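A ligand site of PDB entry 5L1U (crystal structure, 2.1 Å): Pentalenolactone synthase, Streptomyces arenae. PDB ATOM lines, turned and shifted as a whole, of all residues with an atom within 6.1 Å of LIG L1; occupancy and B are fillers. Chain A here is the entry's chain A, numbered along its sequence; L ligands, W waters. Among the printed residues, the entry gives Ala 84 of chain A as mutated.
Water W2 bridges O of Asn 286 (2.7 Å) and O1 of LIG L1 (2.7 Å). Water W1 lies within hydrogen-bond range of O of Thr 391, NH1 of Arg 243, O3 of LIG L1 and ND2 of Asn 286.
The guanidinium group (NH1) of Arg 77 lies within hydrogen-bond range of an oxygen (O2) of LIG L1 (2.9 Å). The guanidinium group (NH2) of Arg 243 lies within salt-bridge range of an oxygen (O1) of LIG L1. O3 of LIG L1 sits close to ND2 of Asn 286, 3.3 Å away.
NH1 of Arg 77 lies within hydrogen-bond range of SD of Met 80 (3.7 Å). The backbone NH (N) of Ile 390 lies within hydrogen-bond range of the backbone carbonyl oxygen (O) of Phe 174. NH1 of Arg 243 is in hydrogen-bond range of O of Thr 239.
SD of Met 80 touches C8 of LIG L1, at 3.7 Å. Phe 235 touches LIG L1. Thr 239 touches LIG L1 (CG2 to C9, 3.6 Å). O of Leu 288 touches C7 of LIG L1, at 3.4 Å. CG1 of Ile 289 touches O5 of LIG L1, 3.8 Å away. Pro 290 touches LIG L1. Ile 390 touches LIG L1 (CG2 to O4, 3.3 Å). Thr 391 touches LIG L1 (CA to O3, 3.4 Å). Hydrophobic or aromatic side chains within 4 Å of LIG L1: Met 80, Phe 235, Ile 289, Pro 290 and Ile 390. Of the 19 residues printed, 11 come within 4 Å of LIG L1. The nearest printed residue that does not touch LIG L1 is Ile 314 (4.8 Å).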
ATOM      1  N   ARG A  77       4.708  16.862  22.830  1.00  0.00           N
ATOM      2  CA  ARG A  77       5.234  17.748  21.789  1.00  0.00           C
ATOM      3  C   ARG A  77       4.884  19.199  22.083  1.00  0.00           C
ATOM      4  O   ARG A  77       5.678  20.105  21.791  1.00  0.00           O
ATOM      5  CB  ARG A  77       4.674  17.379  20.416  1.00  0.00           C
ATOM      6  CG  ARG A  77       5.469  16.334  19.699  1.00  0.00           C
ATOM      7  CD  ARG A  77       6.789  16.890  19.182  1.00  0.00           C
ATOM      8  NE  ARG A  77       7.525  15.816  18.535  1.00  0.00           N
ATOM      9  CZ  ARG A  77       8.808  15.880  18.194  1.00  0.00           C
ATOM     10  NH1 ARG A  77       9.511  16.980  18.444  1.00  0.00           N
ATOM     11  NH2 ARG A  77       9.364  14.837  17.605  1.00  0.00           N
ATOM     12  N   MET A  80       7.339  20.506  24.644  1.00  0.00           N
ATOM     13  CA  MET A  80       8.644  20.690  24.023  1.00  0.00           C
ATOM     14  C   MET A  80       8.706  21.969  23.195  1.00  0.00           C
ATOM     15  O   MET A  80       9.696  22.707  23.244  1.00  0.00           O
ATOM     16  CB  MET A  80       8.986  19.488  23.140  1.00  0.00           C
ATOM     17  CG  MET A  80      10.338  19.597  22.437  1.00  0.00           C
ATOM     18  SD  MET A  80      10.875  18.005  21.781  1.00  0.00           S
ATOM     19  CE  MET A  80      11.241  17.132  23.314  1.00  0.00           C
ATOM     20  N   ALA A  84      10.716  25.736  24.004  1.00  0.00           N
ATOM     21  CA  ALA A  84      11.607  26.356  23.037  1.00  0.00           C
ATOM     22  C   ALA A  84      11.013  27.638  22.437  1.00  0.00           C
ATOM     23  O   ALA A  84      11.443  28.073  21.364  1.00  0.00           O
ATOM     24  CB  ALA A  84      11.967  25.351  21.944  1.00  0.00           C
ATOM     25  N   PHE A 174       8.001  13.942  28.051  1.00  0.00           N
ATOM     26  CA  PHE A 174       8.050  13.724  26.615  1.00  0.00           C
ATOM     27  C   PHE A 174       7.470  12.371  26.211  1.00  0.00           C
ATOM     28  O   PHE A 174       7.797  11.858  25.137  1.00  0.00           O
ATOM     29  CB  PHE A 174       9.479  13.895  26.125  1.00  0.00           C
ATOM     30  CG  PHE A 174      10.016  15.294  26.352  1.00  0.00           C
ATOM     31  CD1 PHE A 174       9.174  16.388  26.268  1.00  0.00           C
ATOM     32  CD2 PHE A 174      11.357  15.500  26.659  1.00  0.00           C
ATOM     33  CE1 PHE A 174       9.654  17.687  26.481  1.00  0.00           C
ATOM     34  CE2 PHE A 174      11.844  16.789  26.879  1.00  0.00           C
ATOM     35  CZ  PHE A 174      10.992  17.873  26.792  1.00  0.00           C
ATOM     36  N   LEU A 234      14.987  19.951  31.146  1.00  0.00           N
ATOM     37  CA  LEU A 234      14.360  18.936  30.305  1.00  0.00           C
ATOM     38  C   LEU A 234      15.110  18.670  29.005  1.00  0.00           C
ATOM     39  O   LEU A 234      15.018  17.551  28.483  1.00  0.00           O
ATOM     40  CB  LEU A 234      12.901  19.325  30.024  1.00  0.00           C
ATOM     41  CG  LEU A 234      11.997  19.386  31.262  1.00  0.00           C
ATOM     42  CD1 LEU A 234      10.666  20.117  31.003  1.00  0.00           C
ATOM     43  CD2 LEU A 234      11.692  17.969  31.787  1.00  0.00           C
ATOM     44  N   PHE A 235      15.855  19.632  28.484  1.00  0.00           N
ATOM     45  CA  PHE A 235      16.698  19.415  27.303  1.00  0.00           C
ATOM     46  C   PHE A 235      18.136  19.041  27.685  1.00  0.00           C
ATOM     47  O   PHE A 235      18.913  18.621  26.807  1.00  0.00           O
ATOM     48  CB  PHE A 235      16.744  20.684  26.422  1.00  0.00           C
ATOM     49  CG  PHE A 235      15.383  21.141  25.893  1.00  0.00           C
ATOM     50  CD1 PHE A 235      14.280  20.275  25.912  1.00  0.00           C
ATOM     51  CD2 PHE A 235      15.221  22.405  25.357  1.00  0.00           C
ATOM     52  CE1 PHE A 235      13.046  20.677  25.423  1.00  0.00           C
ATOM     53  CE2 PHE A 235      13.985  22.829  24.872  1.00  0.00           C
ATOM     54  CZ  PHE A 235      12.891  21.964  24.895  1.00  0.00           C
ATOM     55  N   THR A 239      19.056  13.639  26.523  1.00  0.00           N
ATOM     56  CA  THR A 239      19.668  13.346  25.226  1.00  0.00           C
ATOM     57  C   THR A 239      21.144  12.986  25.368  1.00  0.00           C
ATOM     58  O   THR A 239      21.656  12.163  24.598  1.00  0.00           O
ATOM     59  CB  THR A 239      19.504  14.547  24.273  1.00  0.00           C
ATOM     60  OG1 THR A 239      20.078  15.717  24.867  1.00  0.00           O
ATOM     61  CG2 THR A 239      18.018  14.819  23.964  1.00  0.00           C
ATOM     62  N   ARG A 243      23.179   9.537  24.264  1.00  0.00           N
ATOM     63  CA  ARG A 243      24.390   9.480  23.449  1.00  0.00           C
ATOM     64  C   ARG A 243      25.495   8.677  24.110  1.00  0.00           C
ATOM     65  O   ARG A 243      26.319   8.065  23.405  1.00  0.00           O
ATOM     66  CB  ARG A 243      24.884  10.892  23.122  1.00  0.00           C
ATOM     67  CG  ARG A 243      23.948  11.700  22.188  1.00  0.00           C
ATOM     68  CD  ARG A 243      23.218  10.779  21.218  1.00  0.00           C
ATOM     69  NE  ARG A 243      22.307  11.475  20.305  1.00  0.00           N
ATOM     70  CZ  ARG A 243      21.068  11.832  20.610  1.00  0.00           C
ATOM     71  NH1 ARG A 243      20.587  11.590  21.835  1.00  0.00           N
ATOM     72  NH2 ARG A 243      20.295  12.412  19.699  1.00  0.00           N
ATOM     73  N   SER A 285      13.042   8.400  15.302  1.00  0.00           N
ATOM     74  CA  SER A 285      12.113   9.521  15.209  1.00  0.00           C
ATOM     75  C   SER A 285      12.639  10.761  15.909  1.00  0.00           C
ATOM     76  O   SER A 285      12.189  11.868  15.600  1.00  0.00           O
ATOM     77  CB  SER A 285      10.742   9.139  15.791  1.00  0.00           C
ATOM     78  OG  SER A 285      10.169   8.063  15.066  1.00  0.00           O
ATOM     79  N   ASN A 286      13.589  10.609  16.832  1.00  0.00           N
ATOM     80  CA  ASN A 286      14.195  11.760  17.494  1.00  0.00           C
ATOM     81  C   ASN A 286      15.264  12.419  16.636  1.00  0.00           C
ATOM     82  O   ASN A 286      15.667  13.549  16.936  1.00  0.00           O
ATOM     83  CB  ASN A 286      14.800  11.367  18.836  1.00  0.00           C
ATOM     84  CG  ASN A 286      15.907  10.347  18.680  1.00  0.00           C
ATOM     85  OD1 ASN A 286      15.768   9.364  17.966  1.00  0.00           O
ATOM     86  ND2 ASN A 286      17.021  10.572  19.386  1.00  0.00           N
ATOM     87  N   ALA A 287      15.746  11.744  15.599  1.00  0.00           N
ATOM     88  CA  ALA A 287      16.711  12.312  14.663  1.00  0.00           C
ATOM     89  C   ALA A 287      16.038  13.046  13.517  1.00  0.00           C
ATOM     90  O   ALA A 287      16.564  13.078  12.387  1.00  0.00           O
ATOM     91  CB  ALA A 287      17.648  11.223  14.129  1.00  0.00           C
ATOM     92  N   LEU A 288      14.859  13.599  13.765  1.00  0.00           N
ATOM     93  CA  LEU A 288      14.153  14.470  12.844  1.00  0.00           C
ATOM     94  C   LEU A 288      13.899  15.789  13.555  1.00  0.00           C
ATOM     95  O   LEU A 288      13.394  15.796  14.685  1.00  0.00           O
ATOM     96  CB  LEU A 288      12.822  13.863  12.408  1.00  0.00           C
ATOM     97  CG  LEU A 288      12.787  12.439  11.839  1.00  0.00           C
ATOM     98  CD1 LEU A 288      11.328  12.012  11.635  1.00  0.00           C
ATOM     99  CD2 LEU A 288      13.537  12.377  10.529  1.00  0.00           C
ATOM    100  N   ILE A 289      14.267  16.898  12.928  1.00  0.00           N
ATOM    101  CA  ILE A 289      13.968  18.230  13.447  1.00  0.00           C
ATOM    102  C   ILE A 289      12.712  18.729  12.742  1.00  0.00           C
ATOM    103  O   ILE A 289      12.743  18.911  11.513  1.00  0.00           O
ATOM    104  CB  ILE A 289      15.128  19.205  13.253  1.00  0.00           C
ATOM    105  CG1 ILE A 289      16.346  18.791  14.090  1.00  0.00           C
ATOM    106  CG2 ILE A 289      14.669  20.617  13.604  1.00  0.00           C
ATOM    107  CD1 ILE A 289      17.542  19.725  13.915  1.00  0.00           C
ATOM    108  N   PRO A 290      11.615  18.960  13.464  1.00  0.00           N
ATOM    109  CA  PRO A 290      10.368  19.387  12.808  1.00  0.00           C
ATOM    110  C   PRO A 290      10.313  20.894  12.613  1.00  0.00           C
ATOM    111  O   PRO A 290      10.771  21.685  13.438  1.00  0.00           O
ATOM    112  CB  PRO A 290       9.298  18.936  13.806  1.00  0.00           C
ATOM    113  CG  PRO A 290       9.997  19.088  15.140  1.00  0.00           C
ATOM    114  CD  PRO A 290      11.446  18.748  14.909  1.00  0.00           C
ATOM    115  N   ILE A 314      18.152  14.905  10.323  1.00  0.00           N
ATOM    116  CA  ILE A 314      19.566  15.095  10.640  1.00  0.00           C
ATOM    117  C   ILE A 314      20.278  13.756  10.769  1.00  0.00           C
ATOM    118  O   ILE A 314      21.468  13.646  10.438  1.00  0.00           O
ATOM    119  CB  ILE A 314      19.697  15.950  11.924  1.00  0.00           C
ATOM    120  CG1 ILE A 314      18.965  15.291  13.106  1.00  0.00           C
ATOM    121  CG2 ILE A 314      19.191  17.367  11.686  1.00  0.00           C
ATOM    122  CD1 ILE A 314      19.198  16.018  14.459  1.00  0.00           C
ATOM    123  N   ALA A 342      24.064  16.614  14.251  1.00  0.00           N
ATOM    124  CA  ALA A 342      23.380  16.041  15.423  1.00  0.00           C
ATOM    125  C   ALA A 342      22.989  17.089  16.464  1.00  0.00           C
ATOM    126  O   ALA A 342      22.119  16.801  17.315  1.00  0.00           O
ATOM    127  CB  ALA A 342      24.264  14.986  16.105  1.00  0.00           C
ATOM    128  N   ILE A 390       9.722  11.147  23.019  1.00  0.00           N
ATOM    129  CA  ILE A 390      10.268  11.982  21.944  1.00  0.00           C
ATOM    130  C   ILE A 390      11.771  11.815  21.858  1.00  0.00           C
ATOM    131  O   ILE A 390      12.359  11.797  20.764  1.00  0.00           O
ATOM    132  CB  ILE A 390       9.907  13.466  22.152  1.00  0.00           C
ATOM    133  CG1 ILE A 390       8.392  13.679  22.067  1.00  0.00           C
ATOM    134  CG2 ILE A 390      10.603  14.346  21.112  1.00  0.00           C
ATOM    135  CD1 ILE A 390       7.983  15.078  22.472  1.00  0.00           C
ATOM    136  N   THR A 391      12.419  11.651  23.006  1.00  0.00           N
ATOM    137  CA  THR A 391      13.867  11.496  23.086  1.00  0.00           C
ATOM    138  C   THR A 391      14.325  10.039  22.994  1.00  0.00           C
ATOM    139  O   THR A 391      15.535   9.799  23.097  1.00  0.00           O
ATOM    140  CB  THR A 391      14.368  12.133  24.387  1.00  0.00           C
ATOM    141  OG1 THR A 391      13.511  11.742  25.473  1.00  0.00           O
ATOM    142  CG2 THR A 391      14.333  13.657  24.281  1.00  0.00           C
ATOM    143  N   GLY A 392      13.412   9.088  22.811  1.00  0.00           N
ATOM    144  CA  GLY A 392      13.812   7.702  22.550  1.00  0.00           C
ATOM    145  C   GLY A 392      14.554   7.103  23.730  1.00  0.00           C
ATOM    146  O   GLY A 392      14.126   7.221  24.883  1.00  0.00           O
HETATM  147  C1  LIG L   1      16.802  18.677  21.050  1.00  0.00           C
HETATM  148  C2  LIG L   1      15.448  18.839  21.769  1.00  0.00           C
HETATM  149  C3  LIG L   1      15.229  20.324  22.090  1.00  0.00           C
HETATM  150  C4  LIG L   1      15.411  18.027  23.078  1.00  0.00           C
HETATM  151  C5  LIG L   1      17.260  16.384  20.043  1.00  0.00           C
HETATM  152  C6  LIG L   1      14.144  14.987  19.797  1.00  0.00           C
HETATM  153  C7  LIG L   1      15.399  16.891  17.249  1.00  0.00           C
HETATM  154  C8  LIG L   1      14.422  18.392  20.716  1.00  0.00           C
HETATM  155  C9  LIG L   1      16.807  14.104  20.647  1.00  0.00           C
HETATM  156  C10 LIG L   1      13.214  16.801  18.490  1.00  0.00           C
HETATM  157  C11 LIG L   1      16.422  15.397  20.462  1.00  0.00           C
HETATM  158  C12 LIG L   1      16.597  17.651  19.890  1.00  0.00           C
HETATM  159  C13 LIG L   1      15.111  15.892  20.619  1.00  0.00           C
HETATM  160  C14 LIG L   1      14.541  17.213  18.474  1.00  0.00           C
HETATM  161  C15 LIG L   1      15.119  17.265  19.910  1.00  0.00           C
HETATM  162  O1  LIG L   1      17.956  13.709  20.362  1.00  0.00           O
HETATM  163  O2  LIG L   1      12.349  17.462  17.893  1.00  0.00           O
HETATM  164  O3  LIG L   1      16.040  13.240  21.140  1.00  0.00           O
HETATM  165  O4  LIG L   1      12.953  15.692  19.257  1.00  0.00           O
HETATM  166  O5  LIG L   1      14.915  18.252  17.542  1.00  0.00           O
HETATM  167  C1  LG2 L   2      18.531  22.327  20.907  1.00  0.00           C
HETATM  168  C2  LG2 L   2      20.626  17.980  20.322  1.00  0.00           C
HETATM  169  C3  LG2 L   2      22.537  18.305  24.762  1.00  0.00           C
HETATM  170  C4  LG2 L   2      20.213  22.509  25.485  1.00  0.00           C
HETATM  171  C5  LG2 L   2      18.982  21.172  20.327  1.00  0.00           C
HETATM  172  C6  LG2 L   2      18.754  20.748  18.951  1.00  0.00           C
HETATM  173  C7  LG2 L   2      19.332  19.543  18.794  1.00  0.00           C
HETATM  174  C8  LG2 L   2      19.955  19.161  20.060  1.00  0.00           C
HETATM  175  C9  LG2 L   2      19.350  18.693  17.507  1.00  0.00           C
HETATM  176  C10 LG2 L   2      18.010  21.575  17.870  1.00  0.00           C
HETATM  177  C11 LG2 L   2      16.487  21.468  17.963  1.00  0.00           C
HETATM  178  C12 LG2 L   2      15.814  22.287  16.875  1.00  0.00           C
HETATM  179  O1  LG2 L   2      16.507  22.699  15.905  1.00  0.00           O
HETATM  180  O2  LG2 L   2      14.573  22.526  16.978  1.00  0.00           O
HETATM  181  C13 LG2 L   2      21.329  17.674  21.458  1.00  0.00           C
HETATM  182  C14 LG2 L   2      22.154  16.501  21.684  1.00  0.00           C
HETATM  183  C15 LG2 L   2      22.664  16.599  22.930  1.00  0.00           C
HETATM  184  C16 LG2 L   2      22.198  17.848  23.510  1.00  0.00           C
HETATM  185  C17 LG2 L   2      22.360  15.360  20.651  1.00  0.00           C
HETATM  186  C18 LG2 L   2      23.618  15.658  23.688  1.00  0.00           C
HETATM  187  C19 LG2 L   2      24.580  14.969  23.068  1.00  0.00           C
HETATM  188  C20 LG2 L   2      22.120  19.487  25.341  1.00  0.00           C
HETATM  189  C21 LG2 L   2      22.538  19.986  26.635  1.00  0.00           C
HETATM  190  C22 LG2 L   2      21.892  21.156  26.835  1.00  0.00           C
HETATM  191  C23 LG2 L   2      21.042  21.421  25.678  1.00  0.00           C
HETATM  192  C24 LG2 L   2      23.572  19.253  27.531  1.00  0.00           C
HETATM  193  C25 LG2 L   2      21.960  22.124  28.042  1.00  0.00           C
HETATM  194  C26 LG2 L   2      22.424  21.799  29.264  1.00  0.00           C
HETATM  195  C27 LG2 L   2      19.504  22.793  24.340  1.00  0.00           C
HETATM  196  C28 LG2 L   2      18.532  23.857  24.159  1.00  0.00           C
HETATM  197  C29 LG2 L   2      18.058  23.806  22.908  1.00  0.00           C
HETATM  198  C30 LG2 L   2      18.707  22.703  22.233  1.00  0.00           C
HETATM  199  C31 LG2 L   2      18.114  24.868  25.254  1.00  0.00           C
HETATM  200  C32 LG2 L   2      17.004  24.749  22.293  1.00  0.00           C
HETATM  201  C33 LG2 L   2      17.661  25.611  21.201  1.00  0.00           C
HETATM  202  C34 LG2 L   2      16.648  26.496  20.532  1.00  0.00           C
HETATM  203  O3  LG2 L   2      17.026  27.651  20.202  1.00  0.00           O
HETATM  204  O4  LG2 L   2      15.472  26.061  20.331  1.00  0.00           O
HETATM  205  N1  LG2 L   2      19.717  20.184  20.968  1.00  0.00           N
HETATM  206  N2  LG2 L   2      21.379  18.464  22.599  1.00  0.00           N
HETATM  207  N3  LG2 L   2      21.220  20.380  24.801  1.00  0.00           N
HETATM  208  N4  LG2 L   2      19.579  22.120  23.129  1.00  0.00           N
HETATM  209 FE1  LG2 L   2      20.701  20.432  22.805  1.00  0.00          FE
HETATM  210  O   HOH W   1      17.786  11.360  22.558  1.00  0.00           O
HETATM  211  O   HOH W   2      18.133  14.360  17.721  1.00  0.00           O
